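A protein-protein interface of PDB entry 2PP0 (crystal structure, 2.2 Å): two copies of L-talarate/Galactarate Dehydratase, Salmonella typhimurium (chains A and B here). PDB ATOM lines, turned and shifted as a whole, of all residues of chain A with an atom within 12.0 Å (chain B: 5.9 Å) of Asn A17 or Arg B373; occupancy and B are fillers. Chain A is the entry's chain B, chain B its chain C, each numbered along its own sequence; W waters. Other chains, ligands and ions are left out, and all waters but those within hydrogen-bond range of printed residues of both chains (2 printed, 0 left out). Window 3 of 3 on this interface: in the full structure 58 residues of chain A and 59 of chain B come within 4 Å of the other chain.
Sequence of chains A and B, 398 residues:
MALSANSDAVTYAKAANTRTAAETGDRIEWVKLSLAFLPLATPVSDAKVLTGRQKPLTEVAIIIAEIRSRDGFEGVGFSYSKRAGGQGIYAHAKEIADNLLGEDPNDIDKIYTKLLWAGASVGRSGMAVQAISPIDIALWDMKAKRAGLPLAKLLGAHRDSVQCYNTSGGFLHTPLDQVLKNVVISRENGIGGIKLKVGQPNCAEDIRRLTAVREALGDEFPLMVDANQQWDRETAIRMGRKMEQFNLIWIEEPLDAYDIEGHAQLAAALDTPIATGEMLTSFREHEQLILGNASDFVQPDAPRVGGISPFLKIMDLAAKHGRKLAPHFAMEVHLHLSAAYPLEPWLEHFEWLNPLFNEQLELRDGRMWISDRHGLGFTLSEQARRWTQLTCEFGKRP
No residue of chain A comes within 4 Å of Pro B150.
No residue of chain A comes within 4 Å of Glu B359.
Ser B371 touches just these residues of chain A: Arg A19 and Ala A21.
No residue of chain A comes within 4 Å of His B374.
No residue of chain A comes within 4 Å of Gly B375.
Gly B377 touches none of the printed residues of chain A.
No residue of chain A comes within 4 Å of Phe B378.
Printed residues of chain B within 4 Å of Thr A24: Asp B372.
Printed residues of chain B within 4 Å of Thr A20: Asp B372.
Printed residues of chain B within 4 Å of Arg A146: Leu B149 (3.99 Å).
Leu B376 touches none of the printed residues of chain A.
Leu B361 touches none of the printed residues of chain A.
The nearest residue of chain B that does not touch Asn A17 is Ser B371 (4.8 Å).
The nearest printed residue of chain B that does not touch Thr A20 is Ser B371 (4.03 Å).
ND2 of Asn A17 sits close to N of Arg A19, 2.9 Å away.
The side-chain carboxylate of Glu A23 is in hydrogen-bond range of the backbone NH of Thr A20 (2.9 Å).
The side-chain hydroxyl of Thr A24 sits at hydrogen-bond distance from the backbone carbonyl oxygen of Thr A20.
The side-chain carboxylate of Asp A104 is in hydrogen-bond range of the backbone NH of Asn A106 (2.9 Å).
ND2 of Asn A106 lies close to NE of Arg A146, at 3.3 Å.
OG of Ser B371 lies close to N of Arg B373 (3.2 Å).
No position is printed for both chains.
Gln B360 touches Ala A13.
Gln B360 touches Ala A15.
CB of Asn A17 touches NH1 of Arg B373, 3.5 Å away.
Arg A19 touches Ser B371 (O to CA, 3.4 Å).
Thr A20 touches Asp B372 (C to N, 3.8 Å).
CB of Ala A21 touches O of Ser B371, 3.5 Å away.
Ala A21 touches Asp B372.
OG1 of Thr A24 touches CB of Asp B372 (3.2 Å).
Leu B149 touches Asn A106.
Arg A146 touches Leu B149.
The side-chain amide oxygen (OD1) of Asn A17 lies close to the side-chain carboxylate (OD1) of Asp B372, 3.0 Å away.
The side-chain carboxylate (OD2) of Asp B372 lies within salt-bridge range of the guanidinium group (NE) of Arg A19.
Water W2 bridges N of Ala A16 (2.6 Å) and N of Gln B360 (3.1 Å).
Water W1 lies within hydrogen-bond range of OE2 of Glu B362 (2.8 Å) and O of Arg A19 (3.3 Å).
Printed residues of chain A that touch a printed residue of chain B: Ala A13, Ala A15, Asn A17, Arg A19, Thr A20, Ala A21, Thr A24, Asn A106 and Arg A146.
Of the 16 printed residues of chain B, 5 touch a printed residue of chain A.
Among the printed residues, Asp or Glu carboxylates within 4 Å of a Lys or Arg side-chain nitrogen of the other chain: Arg A19 with Asp B372 (3.9 Å).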
ATOM      1  N   ALA A  13     -11.798  30.299  35.532  1.00  0.00           N
ATOM      2  CA  ALA A  13     -10.716  29.324  35.522  1.00  0.00           C
ATOM      3  C   ALA A  13     -10.215  29.075  34.102  1.00  0.00           C
ATOM      4  O   ALA A  13     -10.648  29.727  33.148  1.00  0.00           O
ATOM      5  CB  ALA A  13     -11.199  28.012  36.144  1.00  0.00           C
ATOM      6  N   LYS A  14      -9.292  28.130  33.973  1.00  0.00           N
ATOM      7  CA  LYS A  14      -8.731  27.762  32.678  1.00  0.00           C
ATOM      8  C   LYS A  14      -8.723  26.242  32.549  1.00  0.00           C
ATOM      9  O   LYS A  14      -8.090  25.540  33.344  1.00  0.00           O
ATOM     10  CB  LYS A  14      -7.309  28.308  32.534  1.00  0.00           C
ATOM     11  CG  LYS A  14      -7.238  29.804  32.278  1.00  0.00           C
ATOM     12  CD  LYS A  14      -7.751  30.147  30.886  1.00  0.00           C
ATOM     13  CE  LYS A  14      -7.630  31.641  30.612  1.00  0.00           C
ATOM     14  NZ  LYS A  14      -8.051  31.997  29.225  1.00  0.00           N
ATOM     15  N   ALA A  15      -9.436  25.740  31.546  1.00  0.00           N
ATOM     16  CA  ALA A  15      -9.522  24.305  31.310  1.00  0.00           C
ATOM     17  C   ALA A  15      -8.213  23.731  30.771  1.00  0.00           C
ATOM     18  O   ALA A  15      -7.600  24.297  29.861  1.00  0.00           O
ATOM     19  CB  ALA A  15     -10.666  24.008  30.339  1.00  0.00           C
ATOM     20  N   ALA A  16      -7.788  22.606  31.345  1.00  0.00           N
ATOM     21  CA  ALA A  16      -6.563  21.932  30.922  1.00  0.00           C
ATOM     22  C   ALA A  16      -6.888  21.077  29.698  1.00  0.00           C
ATOM     23  O   ALA A  16      -6.384  21.329  28.598  1.00  0.00           O
ATOM     24  CB  ALA A  16      -6.027  21.053  32.053  1.00  0.00           C
ATOM     25  N   ASN A  17      -7.736  20.067  29.897  1.00  0.00           N
ATOM     26  CA  ASN A  17      -8.151  19.186  28.808  1.00  0.00           C
ATOM     27  C   ASN A  17      -8.882  20.053  27.785  1.00  0.00           C
ATOM     28  O   ASN A  17      -9.594  20.990  28.151  1.00  0.00           O
ATOM     29  CB  ASN A  17      -9.090  18.089  29.341  1.00  0.00           C
ATOM     30  CG  ASN A  17      -9.467  17.060  28.277  1.00  0.00           C
ATOM     31  OD1 ASN A  17     -10.185  16.097  28.557  1.00  0.00           O
ATOM     32  ND2 ASN A  17      -8.981  17.258  27.055  1.00  0.00           N
ATOM     33  N   THR A  18      -8.702  19.755  26.503  1.00  0.00           N
ATOM     34  CA  THR A  18      -9.353  20.547  25.476  1.00  0.00           C
ATOM     35  C   THR A  18     -10.168  19.702  24.500  1.00  0.00           C
ATOM     36  O   THR A  18     -10.794  20.242  23.587  1.00  0.00           O
ATOM     37  CB  THR A  18      -8.315  21.391  24.696  1.00  0.00           C
ATOM     38  OG1 THR A  18      -7.415  22.018  25.623  1.00  0.00           O
ATOM     39  CG2 THR A  18      -9.015  22.477  23.881  1.00  0.00           C
ATOM     40  N   ARG A  19     -10.172  18.386  24.688  1.00  0.00           N
ATOM     41  CA  ARG A  19     -10.940  17.518  23.799  1.00  0.00           C
ATOM     42  C   ARG A  19     -12.422  17.665  24.133  1.00  0.00           C
ATOM     43  O   ARG A  19     -12.792  17.786  25.302  1.00  0.00           O
ATOM     44  CB  ARG A  19     -10.510  16.060  23.955  1.00  0.00           C
ATOM     45  CG  ARG A  19      -9.024  15.833  23.739  1.00  0.00           C
ATOM     46  CD  ARG A  19      -8.692  14.351  23.689  1.00  0.00           C
ATOM     47  NE  ARG A  19      -9.200  13.731  22.470  1.00  0.00           N
ATOM     48  CZ  ARG A  19      -8.729  13.983  21.250  1.00  0.00           C
ATOM     49  NH1 ARG A  19      -7.733  14.843  21.087  1.00  0.00           N
ATOM     50  NH2 ARG A  19      -9.255  13.378  20.191  1.00  0.00           N
ATOM     51  N   THR A  20     -13.262  17.661  23.103  1.00  0.00           N
ATOM     52  CA  THR A  20     -14.702  17.816  23.289  1.00  0.00           C
ATOM     53  C   THR A  20     -15.458  16.536  22.955  1.00  0.00           C
ATOM     54  O   THR A  20     -14.973  15.696  22.202  1.00  0.00           O
ATOM     55  CB  THR A  20     -15.258  18.942  22.396  1.00  0.00           C
ATOM     56  OG1 THR A  20     -15.120  18.572  21.019  1.00  0.00           O
ATOM     57  CG2 THR A  20     -14.501  20.242  22.638  1.00  0.00           C
ATOM     58  N   ALA A  21     -16.650  16.391  23.524  1.00  0.00           N
ATOM     59  CA  ALA A  21     -17.474  15.219  23.258  1.00  0.00           C
ATOM     60  C   ALA A  21     -17.816  15.193  21.762  1.00  0.00           C
ATOM     61  O   ALA A  21     -17.960  14.128  21.161  1.00  0.00           O
ATOM     62  CB  ALA A  21     -18.755  15.280  24.091  1.00  0.00           C
ATOM     63  N   ALA A  22     -17.933  16.374  21.167  1.00  0.00           N
ATOM     64  CA  ALA A  22     -18.258  16.477  19.750  1.00  0.00           C
ATOM     65  C   ALA A  22     -17.206  15.812  18.865  1.00  0.00           C
ATOM     66  O   ALA A  22     -17.532  15.013  17.990  1.00  0.00           O
ATOM     67  CB  ALA A  22     -18.422  17.946  19.358  1.00  0.00           C
ATOM     68  N   GLU A  23     -15.939  16.127  19.104  1.00  0.00           N
ATOM     69  CA  GLU A  23     -14.867  15.570  18.288  1.00  0.00           C
ATOM     70  C   GLU A  23     -14.470  14.131  18.603  1.00  0.00           C
ATOM     71  O   GLU A  23     -13.936  13.442  17.740  1.00  0.00           O
ATOM     72  CB  GLU A  23     -13.632  16.469  18.382  1.00  0.00           C
ATOM     73  CG  GLU A  23     -12.998  16.509  19.758  1.00  0.00           C
ATOM     74  CD  GLU A  23     -12.097  17.714  19.950  1.00  0.00           C
ATOM     75  OE1 GLU A  23     -11.342  17.735  20.944  1.00  0.00           O
ATOM     76  OE2 GLU A  23     -12.151  18.643  19.114  1.00  0.00           O
ATOM     77  N   THR A  24     -14.743  13.665  19.819  1.00  0.00           N
ATOM     78  CA  THR A  24     -14.354  12.309  20.205  1.00  0.00           C
ATOM     79  C   THR A  24     -15.430  11.231  20.100  1.00  0.00           C
ATOM     80  O   THR A  24     -15.116  10.041  20.091  1.00  0.00           O
ATOM     81  CB  THR A  24     -13.807  12.289  21.652  1.00  0.00           C
ATOM     82  OG1 THR A  24     -14.843  12.679  22.566  1.00  0.00           O
ATOM     83  CG2 THR A  24     -12.640  13.254  21.788  1.00  0.00           C
ATOM     84  N   GLY A  25     -16.694  11.635  20.023  1.00  0.00           N
ATOM     85  CA  GLY A  25     -17.774  10.664  19.948  1.00  0.00           C
ATOM     86  C   GLY A  25     -17.730   9.676  18.792  1.00  0.00           C
ATOM     87  O   GLY A  25     -17.152   9.950  17.740  1.00  0.00           O
ATOM     88  N   ASP A  26     -18.355   8.518  19.000  1.00  0.00           N
ATOM     89  CA  ASP A  26     -18.421   7.467  17.994  1.00  0.00           C
ATOM     90  C   ASP A  26     -19.221   7.983  16.794  1.00  0.00           C
ATOM     91  O   ASP A  26     -19.861   9.036  16.869  1.00  0.00           O
ATOM     92  CB  ASP A  26     -19.098   6.223  18.586  1.00  0.00           C
ATOM     93  CG  ASP A  26     -18.765   4.955  17.821  1.00  0.00           C
ATOM     94  OD1 ASP A  26     -18.141   5.064  16.741  1.00  0.00           O
ATOM     95  OD2 ASP A  26     -19.128   3.850  18.295  1.00  0.00           O
ATOM     96  N   ASP A 104     -23.525  10.722  15.563  1.00  0.00           N
ATOM     97  CA  ASP A 104     -23.073  10.146  16.831  1.00  0.00           C
ATOM     98  C   ASP A 104     -24.256   9.292  17.275  1.00  0.00           C
ATOM     99  O   ASP A 104     -25.299   9.821  17.651  1.00  0.00           O
ATOM    100  CB  ASP A 104     -22.817  11.244  17.864  1.00  0.00           C
ATOM    101  CG  ASP A 104     -22.325  10.695  19.187  1.00  0.00           C
ATOM    102  OD1 ASP A 104     -22.718   9.568  19.544  1.00  0.00           O
ATOM    103  OD2 ASP A 104     -21.557  11.399  19.877  1.00  0.00           O
ATOM    104  N   ASN A 106     -25.095   7.917  19.942  1.00  0.00           N
ATOM    105  CA  ASN A 106     -25.631   8.109  21.284  1.00  0.00           C
ATOM    106  C   ASN A 106     -26.734   9.156  21.378  1.00  0.00           C
ATOM    107  O   ASN A 106     -27.555   9.101  22.288  1.00  0.00           O
ATOM    108  CB  ASN A 106     -24.501   8.457  22.252  1.00  0.00           C
ATOM    109  CG  ASN A 106     -23.446   7.378  22.290  1.00  0.00           C
ATOM    110  OD1 ASN A 106     -22.342   7.553  21.770  1.00  0.00           O
ATOM    111  ND2 ASN A 106     -23.794   6.238  22.874  1.00  0.00           N
ATOM    112  N   ARG A 146     -22.969  -1.004  24.593  1.00  0.00           N
ATOM    113  CA  ARG A 146     -21.820  -0.148  24.856  1.00  0.00           C
ATOM    114  C   ARG A 146     -21.586  -0.054  26.371  1.00  0.00           C
ATOM    115  O   ARG A 146     -20.458   0.111  26.823  1.00  0.00           O
ATOM    116  CB  ARG A 146     -22.059   1.244  24.276  1.00  0.00           C
ATOM    117  CG  ARG A 146     -20.937   2.239  24.523  1.00  0.00           C
ATOM    118  CD  ARG A 146     -21.355   3.642  24.105  1.00  0.00           C
ATOM    119  NE  ARG A 146     -21.672   3.706  22.680  1.00  0.00           N
ATOM    120  CZ  ARG A 146     -20.773   3.909  21.719  1.00  0.00           C
ATOM    121  NH1 ARG A 146     -19.491   4.079  22.029  1.00  0.00           N
ATOM    122  NH2 ARG A 146     -21.152   3.930  20.445  1.00  0.00           N
ATOM    123  N   LEU B 149     -19.011   7.194  28.428  1.00  0.00           N
ATOM    124  CA  LEU B 149     -19.598   8.400  27.857  1.00  0.00           C
ATOM    125  C   LEU B 149     -19.802   9.572  28.803  1.00  0.00           C
ATOM    126  O   LEU B 149     -20.024   9.394  29.996  1.00  0.00           O
ATOM    127  CB  LEU B 149     -20.989   8.096  27.290  1.00  0.00           C
ATOM    128  CG  LEU B 149     -21.281   7.055  26.218  1.00  0.00           C
ATOM    129  CD1 LEU B 149     -22.787   6.825  26.179  1.00  0.00           C
ATOM    130  CD2 LEU B 149     -20.755   7.516  24.869  1.00  0.00           C
ATOM    131  N   PRO B 150     -19.717  10.796  28.270  1.00  0.00           N
ATOM    132  CA  PRO B 150     -19.941  11.965  29.119  1.00  0.00           C
ATOM    133  C   PRO B 150     -21.437  11.784  29.461  1.00  0.00           C
ATOM    134  O   PRO B 150     -22.163  11.169  28.677  1.00  0.00           O
ATOM    135  CB  PRO B 150     -19.709  13.130  28.162  1.00  0.00           C
ATOM    136  CG  PRO B 150     -18.657  12.588  27.224  1.00  0.00           C
ATOM    137  CD  PRO B 150     -19.151  11.180  26.962  1.00  0.00           C
ATOM    138  N   LEU B 151     -21.905  12.285  30.602  1.00  0.00           N
ATOM    139  CA  LEU B 151     -23.315  12.094  30.948  1.00  0.00           C
ATOM    140  C   LEU B 151     -24.276  12.540  29.839  1.00  0.00           C
ATOM    141  O   LEU B 151     -25.256  11.858  29.553  1.00  0.00           O
ATOM    142  CB  LEU B 151     -23.663  12.822  32.248  1.00  0.00           C
ATOM    143  CG  LEU B 151     -25.130  12.708  32.697  1.00  0.00           C
ATOM    144  CD1 LEU B 151     -25.524  11.241  32.894  1.00  0.00           C
ATOM    145  CD2 LEU B 151     -25.328  13.509  33.975  1.00  0.00           C
ATOM    146  N   HIS B 336     -24.793  18.865  31.329  1.00  0.00           N
ATOM    147  CA  HIS B 336     -25.224  17.633  30.680  1.00  0.00           C
ATOM    148  C   HIS B 336     -26.743  17.573  30.486  1.00  0.00           C
ATOM    149  O   HIS B 336     -27.229  17.207  29.413  1.00  0.00           O
ATOM    150  CB  HIS B 336     -24.760  16.434  31.508  1.00  0.00           C
ATOM    151  CG  HIS B 336     -23.270  16.350  31.662  1.00  0.00           C
ATOM    152  ND1 HIS B 336     -22.445  15.868  30.668  1.00  0.00           N
ATOM    153  CD2 HIS B 336     -22.457  16.708  32.685  1.00  0.00           C
ATOM    154  CE1 HIS B 336     -21.188  15.930  31.074  1.00  0.00           C
ATOM    155  NE2 HIS B 336     -21.167  16.437  32.293  1.00  0.00           N
ATOM    156  N   GLU B 359     -10.859  19.572  37.306  1.00  0.00           N
ATOM    157  CA  GLU B 359     -11.101  19.992  35.932  1.00  0.00           C
ATOM    158  C   GLU B 359     -11.984  21.238  35.874  1.00  0.00           C
ATOM    159  O   GLU B 359     -12.781  21.486  36.776  1.00  0.00           O
ATOM    160  CB  GLU B 359     -11.791  18.875  35.141  1.00  0.00           C
ATOM    161  CG  GLU B 359     -11.121  17.513  35.210  1.00  0.00           C
ATOM    162  CD  GLU B 359     -11.382  16.792  36.522  1.00  0.00           C
ATOM    163  OE1 GLU B 359     -12.181  17.304  37.339  1.00  0.00           O
ATOM    164  OE2 GLU B 359     -10.789  15.707  36.729  1.00  0.00           O
ATOM    165  N   GLN B 360     -11.828  22.018  34.810  1.00  0.00           N
ATOM    166  CA  GLN B 360     -12.633  23.219  34.607  1.00  0.00           C
ATOM    167  C   GLN B 360     -13.297  23.121  33.235  1.00  0.00           C
ATOM    168  O   GLN B 360     -12.700  22.610  32.286  1.00  0.00           O
ATOM    169  CB  GLN B 360     -11.754  24.471  34.665  1.00  0.00           C
ATOM    170  CG  GLN B 360     -10.988  24.637  35.978  1.00  0.00           C
ATOM    171  CD  GLN B 360     -11.900  24.602  37.194  1.00  0.00           C
ATOM    172  OE1 GLN B 360     -12.875  25.352  37.277  1.00  0.00           O
ATOM    173  NE2 GLN B 360     -11.586  23.726  38.147  1.00  0.00           N
ATOM    174  N   LEU B 361     -14.534  23.601  33.133  1.00  0.00           N
ATOM    175  CA  LEU B 361     -15.265  23.569  31.870  1.00  0.00           C
ATOM    176  C   LEU B 361     -14.711  24.630  30.926  1.00  0.00           C
ATOM    177  O   LEU B 361     -14.186  25.653  31.364  1.00  0.00           O
ATOM    178  CB  LEU B 361     -16.761  23.820  32.107  1.00  0.00           C
ATOM    179  CG  LEU B 361     -17.535  22.810  32.961  1.00  0.00           C
ATOM    180  CD1 LEU B 361     -18.936  23.345  33.230  1.00  0.00           C
ATOM    181  CD2 LEU B 361     -17.604  21.473  32.248  1.00  0.00           C
ATOM    182  N   GLU B 362     -14.841  24.386  29.627  1.00  0.00           N
ATOM    183  CA  GLU B 362     -14.339  25.310  28.616  1.00  0.00           C
ATOM    184  C   GLU B 362     -15.392  26.317  28.140  1.00  0.00           C
ATOM    185  O   GLU B 362     -16.394  25.940  27.534  1.00  0.00           O
ATOM    186  CB  GLU B 362     -13.808  24.515  27.419  1.00  0.00           C
ATOM    187  CG  GLU B 362     -13.387  25.364  26.224  1.00  0.00           C
ATOM    188  CD  GLU B 362     -12.990  24.520  25.023  1.00  0.00           C
ATOM    189  OE1 GLU B 362     -12.634  25.102  23.975  1.00  0.00           O
ATOM    190  OE2 GLU B 362     -13.037  23.272  25.125  1.00  0.00           O
ATOM    191  N   SER B 371     -16.900  18.426  27.516  1.00  0.00           N
ATOM    192  CA  SER B 371     -15.624  17.769  27.248  1.00  0.00           C
ATOM    193  C   SER B 371     -15.845  16.285  26.962  1.00  0.00           C
ATOM    194  O   SER B 371     -16.963  15.776  27.075  1.00  0.00           O
ATOM    195  CB  SER B 371     -14.672  17.925  28.448  1.00  0.00           C
ATOM    196  OG  SER B 371     -15.009  17.032  29.498  1.00  0.00           O
ATOM    197  N   ASP B 372     -14.774  15.590  26.594  1.00  0.00           N
ATOM    198  CA  ASP B 372     -14.861  14.169  26.309  1.00  0.00           C
ATOM    199  C   ASP B 372     -14.779  13.334  27.588  1.00  0.00           C
ATOM    200  O   ASP B 372     -14.852  12.106  27.533  1.00  0.00           O
ATOM    201  CB  ASP B 372     -13.744  13.760  25.344  1.00  0.00           C
ATOM    202  CG  ASP B 372     -12.367  13.816  25.981  1.00  0.00           C
ATOM    203  OD1 ASP B 372     -12.149  14.681  26.858  1.00  0.00           O
ATOM    204  OD2 ASP B 372     -11.501  13.004  25.587  1.00  0.00           O
ATOM    205  N   ARG B 373     -14.633  13.990  28.737  1.00  0.00           N
ATOM    206  CA  ARG B 373     -14.549  13.268  30.009  1.00  0.00           C
ATOM    207  C   ARG B 373     -15.845  12.513  30.293  1.00  0.00           C
ATOM    208  O   ARG B 373     -16.923  12.955  29.909  1.00  0.00           O
ATOM    209  CB  ARG B 373     -14.221  14.233  31.155  1.00  0.00           C
ATOM    210  CG  ARG B 373     -12.856  14.903  31.008  1.00  0.00           C
ATOM    211  CD  ARG B 373     -12.446  15.648  32.273  1.00  0.00           C
ATOM    212  NE  ARG B 373     -13.273  16.829  32.508  1.00  0.00           N
ATOM    213  CZ  ARG B 373     -13.128  17.985  31.869  1.00  0.00           C
ATOM    214  NH1 ARG B 373     -12.180  18.123  30.951  1.00  0.00           N
ATOM    215  NH2 ARG B 373     -13.934  19.004  32.145  1.00  0.00           N
ATOM    216  N   HIS B 374     -15.737  11.371  30.968  1.00  0.00           N
ATOM    217  CA  HIS B 374     -16.894  10.532  31.267  1.00  0.00           C
ATOM    218  C   HIS B 374     -17.764  10.966  32.446  1.00  0.00           C
ATOM    219  O   HIS B 374     -17.307  11.668  33.352  1.00  0.00           O
ATOM    220  CB  HIS B 374     -16.428   9.090  31.465  1.00  0.00           C
ATOM    221  CG  HIS B 374     -15.712   8.530  30.276  1.00  0.00           C
ATOM    222  ND1 HIS B 374     -15.130   7.281  30.275  1.00  0.00           N
ATOM    223  CD2 HIS B 374     -15.509   9.040  29.037  1.00  0.00           C
ATOM    224  CE1 HIS B 374     -14.604   7.044  29.088  1.00  0.00           C
ATOM    225  NE2 HIS B 374     -14.821   8.096  28.317  1.00  0.00           N
ATOM    226  N   GLY B 375     -19.025  10.530  32.422  1.00  0.00           N
ATOM    227  CA  GLY B 375     -19.960  10.893  33.472  1.00  0.00           C
ATOM    228  C   GLY B 375     -20.043  12.404  33.570  1.00  0.00           C
ATOM    229  O   GLY B 375     -20.082  13.096  32.550  1.00  0.00           O
ATOM    230  N   LEU B 376     -20.059  12.923  34.792  1.00  0.00           N
ATOM    231  CA  LEU B 376     -20.118  14.364  34.991  1.00  0.00           C
ATOM    232  C   LEU B 376     -18.837  15.018  34.468  1.00  0.00           C
ATOM    233  O   LEU B 376     -18.818  16.210  34.164  1.00  0.00           O
ATOM    234  CB  LEU B 376     -20.317  14.681  36.472  1.00  0.00           C
ATOM    235  CG  LEU B 376     -21.591  14.095  37.091  1.00  0.00           C
ATOM    236  CD1 LEU B 376     -21.586  14.322  38.593  1.00  0.00           C
ATOM    237  CD2 LEU B 376     -22.819  14.738  36.454  1.00  0.00           C
ATOM    238  N   GLY B 377     -17.771  14.228  34.355  1.00  0.00           N
ATOM    239  CA  GLY B 377     -16.508  14.746  33.858  1.00  0.00           C
ATOM    240  C   GLY B 377     -15.663  15.480  34.890  1.00  0.00           C
ATOM    241  O   GLY B 377     -14.802  16.291  34.530  1.00  0.00           O
ATOM    242  N   PHE B 378     -15.895  15.209  36.171  1.00  0.00           N
ATOM    243  CA  PHE B 378     -15.130  15.868  37.227  1.00  0.00           C
ATOM    244  C   PHE B 378     -14.587  14.897  38.263  1.00  0.00           C
ATOM    245  O   PHE B 378     -15.179  13.846  38.516  1.00  0.00           O
ATOM    246  CB  PHE B 378     -15.996  16.909  37.946  1.00  0.00           C
ATOM    247  CG  PHE B 378     -16.332  18.108  37.107  1.00  0.00           C
ATOM    248  CD1 PHE B 378     -15.409  19.139  36.937  1.00  0.00           C
ATOM    249  CD2 PHE B 378     -17.569  18.208  36.476  1.00  0.00           C
ATOM    250  CE1 PHE B 378     -15.713  20.254  36.152  1.00  0.00           C
ATOM    251  CE2 PHE B 378     -17.882  19.318  35.688  1.00  0.00           C
ATOM    252  CZ  PHE B 378     -16.952  20.341  35.527  1.00  0.00           C
HETATM  253  O   HOH W   1     -13.980  20.799  25.994  1.00  0.00           O
HETATM  254  O   HOH W   2      -9.371  21.329  33.034  1.00  0.00           O
